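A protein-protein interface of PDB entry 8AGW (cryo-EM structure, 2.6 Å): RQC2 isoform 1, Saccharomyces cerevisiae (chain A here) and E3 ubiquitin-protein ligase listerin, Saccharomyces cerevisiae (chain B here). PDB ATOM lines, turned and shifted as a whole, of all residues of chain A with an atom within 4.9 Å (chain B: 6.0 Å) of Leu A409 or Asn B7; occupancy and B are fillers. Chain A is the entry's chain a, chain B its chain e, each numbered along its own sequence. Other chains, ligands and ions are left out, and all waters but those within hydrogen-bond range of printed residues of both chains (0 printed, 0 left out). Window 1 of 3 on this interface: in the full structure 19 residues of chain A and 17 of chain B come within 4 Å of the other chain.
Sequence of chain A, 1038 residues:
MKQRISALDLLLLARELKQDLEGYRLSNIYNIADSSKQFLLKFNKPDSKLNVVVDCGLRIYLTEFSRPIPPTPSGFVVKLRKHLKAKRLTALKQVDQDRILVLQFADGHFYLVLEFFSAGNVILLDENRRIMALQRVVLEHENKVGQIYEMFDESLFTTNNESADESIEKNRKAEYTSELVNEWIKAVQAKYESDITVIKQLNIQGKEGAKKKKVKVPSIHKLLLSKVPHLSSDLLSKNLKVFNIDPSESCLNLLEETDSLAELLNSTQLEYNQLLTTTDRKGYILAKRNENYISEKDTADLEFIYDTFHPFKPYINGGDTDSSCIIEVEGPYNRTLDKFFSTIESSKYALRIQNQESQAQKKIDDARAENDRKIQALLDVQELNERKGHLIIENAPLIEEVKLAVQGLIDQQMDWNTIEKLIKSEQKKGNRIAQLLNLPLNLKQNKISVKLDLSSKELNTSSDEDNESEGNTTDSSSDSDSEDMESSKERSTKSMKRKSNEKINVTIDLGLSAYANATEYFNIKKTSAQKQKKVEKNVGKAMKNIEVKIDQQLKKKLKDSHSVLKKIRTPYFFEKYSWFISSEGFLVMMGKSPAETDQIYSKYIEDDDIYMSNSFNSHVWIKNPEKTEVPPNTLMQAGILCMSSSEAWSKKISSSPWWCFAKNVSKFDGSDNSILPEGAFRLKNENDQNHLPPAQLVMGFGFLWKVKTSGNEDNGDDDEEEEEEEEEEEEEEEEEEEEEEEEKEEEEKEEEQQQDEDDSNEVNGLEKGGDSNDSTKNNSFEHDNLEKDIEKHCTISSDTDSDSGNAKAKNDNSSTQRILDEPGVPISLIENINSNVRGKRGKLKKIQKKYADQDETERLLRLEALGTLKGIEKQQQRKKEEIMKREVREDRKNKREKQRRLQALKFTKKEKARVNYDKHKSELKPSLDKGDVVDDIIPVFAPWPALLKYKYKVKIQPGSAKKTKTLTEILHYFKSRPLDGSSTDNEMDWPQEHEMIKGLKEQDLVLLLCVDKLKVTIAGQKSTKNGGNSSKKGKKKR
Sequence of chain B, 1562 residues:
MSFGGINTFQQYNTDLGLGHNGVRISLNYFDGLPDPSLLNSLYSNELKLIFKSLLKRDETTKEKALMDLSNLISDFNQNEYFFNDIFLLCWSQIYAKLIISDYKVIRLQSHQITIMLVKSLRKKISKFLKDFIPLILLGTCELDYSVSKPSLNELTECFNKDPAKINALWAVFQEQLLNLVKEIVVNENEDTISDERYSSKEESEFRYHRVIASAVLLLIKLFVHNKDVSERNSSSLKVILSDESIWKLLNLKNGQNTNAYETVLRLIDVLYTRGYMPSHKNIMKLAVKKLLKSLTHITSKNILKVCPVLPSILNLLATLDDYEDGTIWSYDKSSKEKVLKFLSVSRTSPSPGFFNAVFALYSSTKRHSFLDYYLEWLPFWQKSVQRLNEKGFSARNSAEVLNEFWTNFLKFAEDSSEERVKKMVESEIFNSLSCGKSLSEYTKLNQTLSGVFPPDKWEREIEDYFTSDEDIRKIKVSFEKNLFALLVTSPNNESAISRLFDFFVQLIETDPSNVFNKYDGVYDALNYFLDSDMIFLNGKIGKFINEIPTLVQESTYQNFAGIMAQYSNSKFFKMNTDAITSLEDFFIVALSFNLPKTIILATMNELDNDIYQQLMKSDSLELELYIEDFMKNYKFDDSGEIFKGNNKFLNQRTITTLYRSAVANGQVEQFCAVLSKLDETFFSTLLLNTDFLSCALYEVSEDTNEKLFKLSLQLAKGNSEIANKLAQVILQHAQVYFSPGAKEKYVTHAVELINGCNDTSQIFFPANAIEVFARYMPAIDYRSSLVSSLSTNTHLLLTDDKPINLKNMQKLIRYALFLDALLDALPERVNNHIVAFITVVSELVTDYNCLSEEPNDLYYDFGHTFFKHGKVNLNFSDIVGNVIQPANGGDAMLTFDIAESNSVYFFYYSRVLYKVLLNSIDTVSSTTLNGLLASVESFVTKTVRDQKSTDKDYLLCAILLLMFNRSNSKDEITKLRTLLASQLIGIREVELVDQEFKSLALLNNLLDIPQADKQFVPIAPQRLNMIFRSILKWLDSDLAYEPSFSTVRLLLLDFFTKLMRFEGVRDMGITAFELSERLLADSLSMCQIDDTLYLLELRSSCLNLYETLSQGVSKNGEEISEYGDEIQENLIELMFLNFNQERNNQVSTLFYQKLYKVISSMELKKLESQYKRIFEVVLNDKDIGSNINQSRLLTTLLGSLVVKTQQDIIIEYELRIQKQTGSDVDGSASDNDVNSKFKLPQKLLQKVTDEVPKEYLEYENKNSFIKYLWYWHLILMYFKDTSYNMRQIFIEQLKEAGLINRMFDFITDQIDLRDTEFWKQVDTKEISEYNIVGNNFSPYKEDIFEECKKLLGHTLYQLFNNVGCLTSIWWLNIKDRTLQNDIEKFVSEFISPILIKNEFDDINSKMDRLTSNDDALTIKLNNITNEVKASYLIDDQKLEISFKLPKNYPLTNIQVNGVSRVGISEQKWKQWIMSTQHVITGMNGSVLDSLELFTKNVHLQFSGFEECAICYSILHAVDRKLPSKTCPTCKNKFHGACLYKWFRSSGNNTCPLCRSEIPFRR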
ATOM      1  N   ALA A 405       0.069 -31.931   7.811  1.00  0.00           N
ATOM      2  CA  ALA A 405       1.061 -31.770   6.754  1.00  0.00           C
ATOM      3  C   ALA A 405       0.431 -31.295   5.446  1.00  0.00           C
ATOM      4  O   ALA A 405       0.907 -30.328   4.832  1.00  0.00           O
ATOM      5  CB  ALA A 405       1.810 -33.083   6.553  1.00  0.00           C
ATOM      6  N   VAL A 406      -0.654 -31.949   5.019  1.00  0.00           N
ATOM      7  CA  VAL A 406      -1.306 -31.583   3.762  1.00  0.00           C
ATOM      8  C   VAL A 406      -1.928 -30.195   3.867  1.00  0.00           C
ATOM      9  O   VAL A 406      -1.858 -29.399   2.925  1.00  0.00           O
ATOM     10  CB  VAL A 406      -2.339 -32.654   3.359  1.00  0.00           C
ATOM     11  CG1 VAL A 406      -3.052 -32.278   2.068  1.00  0.00           C
ATOM     12  CG2 VAL A 406      -1.657 -33.991   3.173  1.00  0.00           C
ATOM     13  N   GLN A 407      -2.492 -29.859   5.031  1.00  0.00           N
ATOM     14  CA  GLN A 407      -3.061 -28.531   5.222  1.00  0.00           C
ATOM     15  C   GLN A 407      -1.988 -27.453   5.271  1.00  0.00           C
ATOM     16  O   GLN A 407      -2.226 -26.332   4.807  1.00  0.00           O
ATOM     17  CB  GLN A 407      -3.900 -28.503   6.496  1.00  0.00           C
ATOM     18  CG  GLN A 407      -4.825 -27.312   6.593  1.00  0.00           C
ATOM     19  CD  GLN A 407      -6.087 -27.502   5.786  1.00  0.00           C
ATOM     20  OE1 GLN A 407      -6.356 -26.754   4.847  1.00  0.00           O
ATOM     21  NE2 GLN A 407      -6.870 -28.512   6.142  1.00  0.00           N
ATOM     22  N   GLY A 408      -0.805 -27.767   5.807  1.00  0.00           N
ATOM     23  CA  GLY A 408       0.291 -26.815   5.755  1.00  0.00           C
ATOM     24  C   GLY A 408       0.779 -26.566   4.341  1.00  0.00           C
ATOM     25  O   GLY A 408       1.136 -25.440   3.989  1.00  0.00           O
ATOM     26  N   LEU A 409       0.802 -27.612   3.511  1.00  0.00           N
ATOM     27  CA  LEU A 409       1.119 -27.397   2.099  1.00  0.00           C
ATOM     28  C   LEU A 409       0.015 -26.638   1.370  1.00  0.00           C
ATOM     29  O   LEU A 409       0.296 -25.878   0.436  1.00  0.00           O
ATOM     30  CB  LEU A 409       1.427 -28.718   1.390  1.00  0.00           C
ATOM     31  CG  LEU A 409       2.842 -29.308   1.466  1.00  0.00           C
ATOM     32  CD1 LEU A 409       3.761 -28.335   0.768  1.00  0.00           C
ATOM     33  CD2 LEU A 409       3.386 -29.578   2.851  1.00  0.00           C
ATOM     34  N   ILE A 410      -1.244 -26.844   1.764  1.00  0.00           N
ATOM     35  CA  ILE A 410      -2.357 -26.127   1.142  1.00  0.00           C
ATOM     36  C   ILE A 410      -2.315 -24.645   1.494  1.00  0.00           C
ATOM     37  O   ILE A 410      -2.514 -23.780   0.632  1.00  0.00           O
ATOM     38  CB  ILE A 410      -3.694 -26.786   1.538  1.00  0.00           C
ATOM     39  CG1 ILE A 410      -3.891 -28.082   0.751  1.00  0.00           C
ATOM     40  CG2 ILE A 410      -4.877 -25.852   1.351  1.00  0.00           C
ATOM     41  CD1 ILE A 410      -5.174 -28.799   1.072  1.00  0.00           C
ATOM     42  N   ASP A 411      -1.983 -24.326   2.747  1.00  0.00           N
ATOM     43  CA  ASP A 411      -1.985 -22.945   3.218  1.00  0.00           C
ATOM     44  C   ASP A 411      -0.853 -22.105   2.642  1.00  0.00           C
ATOM     45  O   ASP A 411      -0.851 -20.888   2.840  1.00  0.00           O
ATOM     46  CB  ASP A 411      -1.915 -22.917   4.742  1.00  0.00           C
ATOM     47  CG  ASP A 411      -3.192 -23.404   5.386  1.00  0.00           C
ATOM     48  OD1 ASP A 411      -4.204 -23.541   4.668  1.00  0.00           O
ATOM     49  OD2 ASP A 411      -3.185 -23.655   6.608  1.00  0.00           O
ATOM     50  N   GLN A 412       0.095 -22.711   1.935  1.00  0.00           N
ATOM     51  CA  GLN A 412       1.100 -21.978   1.182  1.00  0.00           C
ATOM     52  C   GLN A 412       0.604 -21.562  -0.194  1.00  0.00           C
ATOM     53  O   GLN A 412       1.391 -20.992  -0.960  1.00  0.00           O
ATOM     54  CB  GLN A 412       2.367 -22.823   1.035  1.00  0.00           C
ATOM     55  CG  GLN A 412       2.985 -23.227   2.352  1.00  0.00           C
ATOM     56  CD  GLN A 412       4.204 -24.101   2.178  1.00  0.00           C
ATOM     57  OE1 GLN A 412       4.852 -24.081   1.133  1.00  0.00           O
ATOM     58  NE2 GLN A 412       4.521 -24.884   3.203  1.00  0.00           N
ATOM     59  N   GLN A 413      -0.672 -21.838  -0.502  1.00  0.00           N
ATOM     60  CA  GLN A 413      -1.301 -21.572  -1.803  1.00  0.00           C
ATOM     61  C   GLN A 413      -0.537 -22.250  -2.934  1.00  0.00           C
ATOM     62  O   GLN A 413      -0.315 -21.669  -3.997  1.00  0.00           O
ATOM     63  CB  GLN A 413      -1.457 -20.073  -2.062  1.00  0.00           C
ATOM     64  CG  GLN A 413      -2.666 -19.459  -1.398  1.00  0.00           C
ATOM     65  CD  GLN A 413      -2.929 -18.056  -1.887  1.00  0.00           C
ATOM     66  OE1 GLN A 413      -2.637 -17.083  -1.196  1.00  0.00           O
ATOM     67  NE2 GLN A 413      -3.469 -17.943  -3.093  1.00  0.00           N
ATOM     68  N   MET A 414      -0.112 -23.482  -2.689  1.00  0.00           N
ATOM     69  CA  MET A 414       0.703 -24.204  -3.644  1.00  0.00           C
ATOM     70  C   MET A 414      -0.198 -24.946  -4.624  1.00  0.00           C
ATOM     71  O   MET A 414      -1.316 -25.345  -4.286  1.00  0.00           O
ATOM     72  CB  MET A 414       1.638 -25.160  -2.897  1.00  0.00           C
ATOM     73  CG  MET A 414       2.660 -25.910  -3.733  1.00  0.00           C
ATOM     74  SD  MET A 414       3.695 -26.979  -2.724  1.00  0.00           S
ATOM     75  CE  MET A 414       4.696 -25.752  -1.887  1.00  0.00           C
ATOM     76  N   ILE A 419       1.883 -30.245  -5.494  1.00  0.00           N
ATOM     77  CA  ILE A 419       1.758 -30.942  -4.217  1.00  0.00           C
ATOM     78  C   ILE A 419       1.778 -32.453  -4.423  1.00  0.00           C
ATOM     79  O   ILE A 419       2.459 -33.171  -3.678  1.00  0.00           O
ATOM     80  CB  ILE A 419       0.489 -30.477  -3.477  1.00  0.00           C
ATOM     81  CG1 ILE A 419       0.661 -29.043  -2.981  1.00  0.00           C
ATOM     82  CG2 ILE A 419       0.156 -31.383  -2.301  1.00  0.00           C
ATOM     83  CD1 ILE A 419      -0.549 -28.494  -2.251  1.00  0.00           C
ATOM     84  N   LEU A 422       5.291 -33.453  -5.136  1.00  0.00           N
ATOM     85  CA  LEU A 422       6.006 -33.467  -3.867  1.00  0.00           C
ATOM     86  C   LEU A 422       5.690 -34.706  -3.040  1.00  0.00           C
ATOM     87  O   LEU A 422       6.575 -35.210  -2.340  1.00  0.00           O
ATOM     88  CB  LEU A 422       5.669 -32.204  -3.076  1.00  0.00           C
ATOM     89  CG  LEU A 422       6.399 -31.991  -1.751  1.00  0.00           C
ATOM     90  CD1 LEU A 422       7.891 -31.974  -1.971  1.00  0.00           C
ATOM     91  CD2 LEU A 422       5.950 -30.710  -1.097  1.00  0.00           C
ATOM     92  N   GLY B   5       1.466 -20.679   5.761  1.00  0.00           N
ATOM     93  CA  GLY B   5       1.717 -22.095   5.577  1.00  0.00           C
ATOM     94  C   GLY B   5       3.002 -22.618   6.170  1.00  0.00           C
ATOM     95  O   GLY B   5       3.901 -21.841   6.466  1.00  0.00           O
ATOM     96  N   ILE B   6       3.080 -23.927   6.385  1.00  0.00           N
ATOM     97  CA  ILE B   6       4.263 -24.533   6.989  1.00  0.00           C
ATOM     98  C   ILE B   6       4.756 -25.708   6.158  1.00  0.00           C
ATOM     99  O   ILE B   6       3.951 -26.518   5.711  1.00  0.00           O
ATOM    100  CB  ILE B   6       3.939 -25.041   8.406  1.00  0.00           C
ATOM    101  CG1 ILE B   6       3.601 -23.877   9.337  1.00  0.00           C
ATOM    102  CG2 ILE B   6       5.104 -25.817   8.999  1.00  0.00           C
ATOM    103  CD1 ILE B   6       4.781 -22.979   9.639  1.00  0.00           C
ATOM    104  N   ASN B   7       6.060 -25.817   5.938  1.00  0.00           N
ATOM    105  CA  ASN B   7       6.589 -26.979   5.226  1.00  0.00           C
ATOM    106  C   ASN B   7       6.815 -28.140   6.175  1.00  0.00           C
ATOM    107  O   ASN B   7       7.955 -28.485   6.472  1.00  0.00           O
ATOM    108  CB  ASN B   7       7.894 -26.636   4.521  1.00  0.00           C
ATOM    109  CG  ASN B   7       7.682 -26.139   3.107  1.00  0.00           C
ATOM    110  OD1 ASN B   7       6.802 -26.621   2.395  1.00  0.00           O
ATOM    111  ND2 ASN B   7       8.498 -25.182   2.688  1.00  0.00           N
ATOM    112  N   THR B   8       5.737 -28.752   6.647  1.00  0.00           N
ATOM    113  CA  THR B   8       5.848 -29.862   7.586  1.00  0.00           C
ATOM    114  C   THR B   8       6.537 -31.077   6.996  1.00  0.00           C
ATOM    115  O   THR B   8       7.325 -31.730   7.674  1.00  0.00           O
ATOM    116  CB  THR B   8       4.477 -30.265   8.130  1.00  0.00           C
ATOM    117  OG1 THR B   8       3.512 -29.275   7.756  1.00  0.00           O
ATOM    118  CG2 THR B   8       4.519 -30.379   9.641  1.00  0.00           C
ATOM    119  N   PHE B   9       6.260 -31.381   5.732  1.00  0.00           N
ATOM    120  CA  PHE B   9       6.839 -32.564   5.104  1.00  0.00           C
ATOM    121  C   PHE B   9       8.348 -32.471   5.087  1.00  0.00           C
ATOM    122  O   PHE B   9       9.038 -33.462   5.315  1.00  0.00           O
ATOM    123  CB  PHE B   9       6.332 -32.711   3.674  1.00  0.00           C
ATOM    124  CG  PHE B   9       5.133 -33.591   3.549  1.00  0.00           C
ATOM    125  CD1 PHE B   9       5.264 -34.961   3.615  1.00  0.00           C
ATOM    126  CD2 PHE B   9       3.878 -33.051   3.361  1.00  0.00           C
ATOM    127  CE1 PHE B   9       4.164 -35.778   3.499  1.00  0.00           C
ATOM    128  CE2 PHE B   9       2.771 -33.862   3.242  1.00  0.00           C
ATOM    129  CZ  PHE B   9       2.913 -35.230   3.318  1.00  0.00           C
ATOM    130  N   GLN B  10       8.866 -31.282   4.828  1.00  0.00           N
ATOM    131  CA  GLN B  10      10.307 -31.092   4.756  1.00  0.00           C
ATOM    132  C   GLN B  10      11.010 -31.394   6.065  1.00  0.00           C
ATOM    133  O   GLN B  10      12.124 -31.910   6.063  1.00  0.00           O
ATOM    134  CB  GLN B  10      10.632 -29.675   4.292  1.00  0.00           C
ATOM    135  CG  GLN B  10       9.970 -29.299   2.976  1.00  0.00           C
ATOM    136  CD  GLN B  10      10.404 -30.176   1.817  1.00  0.00           C
ATOM    137  OE1 GLN B  10      11.568 -30.563   1.713  1.00  0.00           O
ATOM    138  NE2 GLN B  10       9.467 -30.482   0.929  1.00  0.00           N
ATOM    139  N   GLN B  11      10.377 -31.075   7.184  1.00  0.00           N
ATOM    140  CA  GLN B  11      11.028 -31.258   8.473  1.00  0.00           C
ATOM    141  C   GLN B  11      11.405 -32.703   8.705  1.00  0.00           C
ATOM    142  O   GLN B  11      12.476 -32.992   9.229  1.00  0.00           O
ATOM    143  CB  GLN B  11      10.084 -30.822   9.585  1.00  0.00           C
ATOM    144  CG  GLN B  11       9.538 -29.418   9.407  1.00  0.00           C
ATOM    145  CD  GLN B  11       8.325 -29.161  10.274  1.00  0.00           C
ATOM    146  OE1 GLN B  11       7.857 -30.052  10.982  1.00  0.00           O
ATOM    147  NE2 GLN B  11       7.803 -27.942  10.216  1.00  0.00           N
ATOM    148  N   LEU B  33      11.585 -24.685  -2.221  1.00  0.00           N
ATOM    149  CA  LEU B  33      11.015 -23.352  -2.252  1.00  0.00           C
ATOM    150  C   LEU B  33      11.175 -22.725  -0.891  1.00  0.00           C
ATOM    151  O   LEU B  33      11.136 -23.421   0.117  1.00  0.00           O
ATOM    152  CB  LEU B  33       9.547 -23.442  -2.626  1.00  0.00           C
ATOM    153  CG  LEU B  33       9.262 -23.838  -4.070  1.00  0.00           C
ATOM    154  CD1 LEU B  33       7.803 -24.229  -4.237  1.00  0.00           C
ATOM    155  CD2 LEU B  33       9.628 -22.691  -4.997  1.00  0.00           C
ATOM    156  N   PRO B  34      11.351 -21.404  -0.841  1.00  0.00           N
ATOM    157  CA  PRO B  34      11.619 -20.801   0.464  1.00  0.00           C
ATOM    158  C   PRO B  34      10.475 -20.996   1.440  1.00  0.00           C
ATOM    159  O   PRO B  34       9.316 -20.893   1.052  1.00  0.00           O
ATOM    160  CB  PRO B  34      11.797 -19.329   0.129  1.00  0.00           C
ATOM    161  CG  PRO B  34      12.216 -19.303  -1.297  1.00  0.00           C
ATOM    162  CD  PRO B  34      11.477 -20.433  -1.940  1.00  0.00           C
ATOM    163  N   ASP B  35      10.793 -21.281   2.693  1.00  0.00           N
ATOM    164  CA  ASP B  35       9.770 -21.526   3.704  1.00  0.00           C
ATOM    165  C   ASP B  35       9.006 -20.267   4.000  1.00  0.00           C
ATOM    166  O   ASP B  35       9.587 -19.192   4.050  1.00  0.00           O
ATOM    167  CB  ASP B  35      10.429 -22.006   4.990  1.00  0.00           C
ATOM    168  CG  ASP B  35       9.459 -22.675   5.931  1.00  0.00           C
ATOM    169  OD1 ASP B  35       8.759 -23.608   5.494  1.00  0.00           O
ATOM    170  OD2 ASP B  35       9.404 -22.281   7.113  1.00  0.00           O
ATOM    171  N   PRO B  36       7.705 -20.386   4.234  1.00  0.00           N
ATOM    172  CA  PRO B  36       6.947 -19.158   4.422  1.00  0.00           C
ATOM    173  C   PRO B  36       7.404 -18.322   5.608  1.00  0.00           C
ATOM    174  O   PRO B  36       7.422 -17.099   5.523  1.00  0.00           O
ATOM    175  CB  PRO B  36       5.550 -19.680   4.651  1.00  0.00           C
ATOM    176  CG  PRO B  36       5.486 -20.861   3.755  1.00  0.00           C
ATOM    177  CD  PRO B  36       6.825 -21.517   3.905  1.00  0.00           C
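NE2 of Gln A412 sits at hydrogen-bond distance from OD1 of Asn B7, 3.0 Å away.
N of Ile B6 lies within hydrogen-bond range of O of Gly A408 (3.4 Å).
The side-chain amide nitrogen of Gln A412 lies within hydrogen-bond range of the backbone carbonyl oxygen of Ile B6, at 3.0 Å.
The side-chain amide nitrogen (ND2) of Asn B7 lies within hydrogen-bond range of the side-chain carboxylate (OD1) of Asp B35 (3.2 Å).
The side-chain hydroxyl of Thr B8 lies within hydrogen-bond range of the backbone carbonyl oxygen of Ile B6, 3.5 Å away.
Ala A405 touches Thr B8 (CA to OG1, 3.6 Å).
Ala A405 touches Phe B9.
Gly A408 touches Gly B5 (O to CA, 3.7 Å).
Leu A409 touches Ile B6 (N to O, 3.99 Å).
Leu A409 touches Asn B7 (CD1 to OD1, 3.9 Å).
CD2 of Phe B9 touches CD2 of Leu A409, at 3.5 Å.
N of Gly B5 touches O of Asp A411, 3.7 Å away.
CA of Gly B5 touches CG of Gln A412, 3.6 Å away.
Gln A412 touches Pro B36.
Leu A422 touches Gln B10 (CD1 to NE2, 3.6 Å).
Val A406 touches none of the printed residues of chain B.
Printed residues of chain B within 4 Å of Gly A408: Gly B5 (3.7 Å) and Ile B6 (3.4 Å).
Printed residues of chain B within 4 Å of Leu A409: Ile B6, Asn B7 and Phe B9.
Of the printed residues of chain B, Gln A412 touches Gly B5 (3.6 Å), Ile B6 (3.0 Å), Asn B7 (3.0 Å) and Pro B36 (3.7 Å).
Printed residues of chain A within 4 Å of Gly B5: Gly A408, Asp A411 and Gln A412.
Printed residues of chain A within 4 Å of Ile B6: Gly A408 (3.4 Å), Leu A409 (3.99 Å) and Gln A412 (3.0 Å).
Asn B7 touches just these residues of chain A: Leu A409 and Gln A412.
Gln B11 touches none of the printed residues of chain A.
The nearest printed residue of chain A that does not touch Asn B7 is Met A414 (4.9 Å).
Of the 11 printed residues of chain B, 7 touch a printed residue of chain A.
Printed residues of chain B that touch a printed residue of chain A: Gly B5, Ile B6, Asn B7, Thr B8, Phe B9, Gln B10 and Pro B36.
Among the printed residues, no Asp or Glu carboxylate lies within 4 Å of a Lys or Arg side-chain nitrogen of the other chain.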
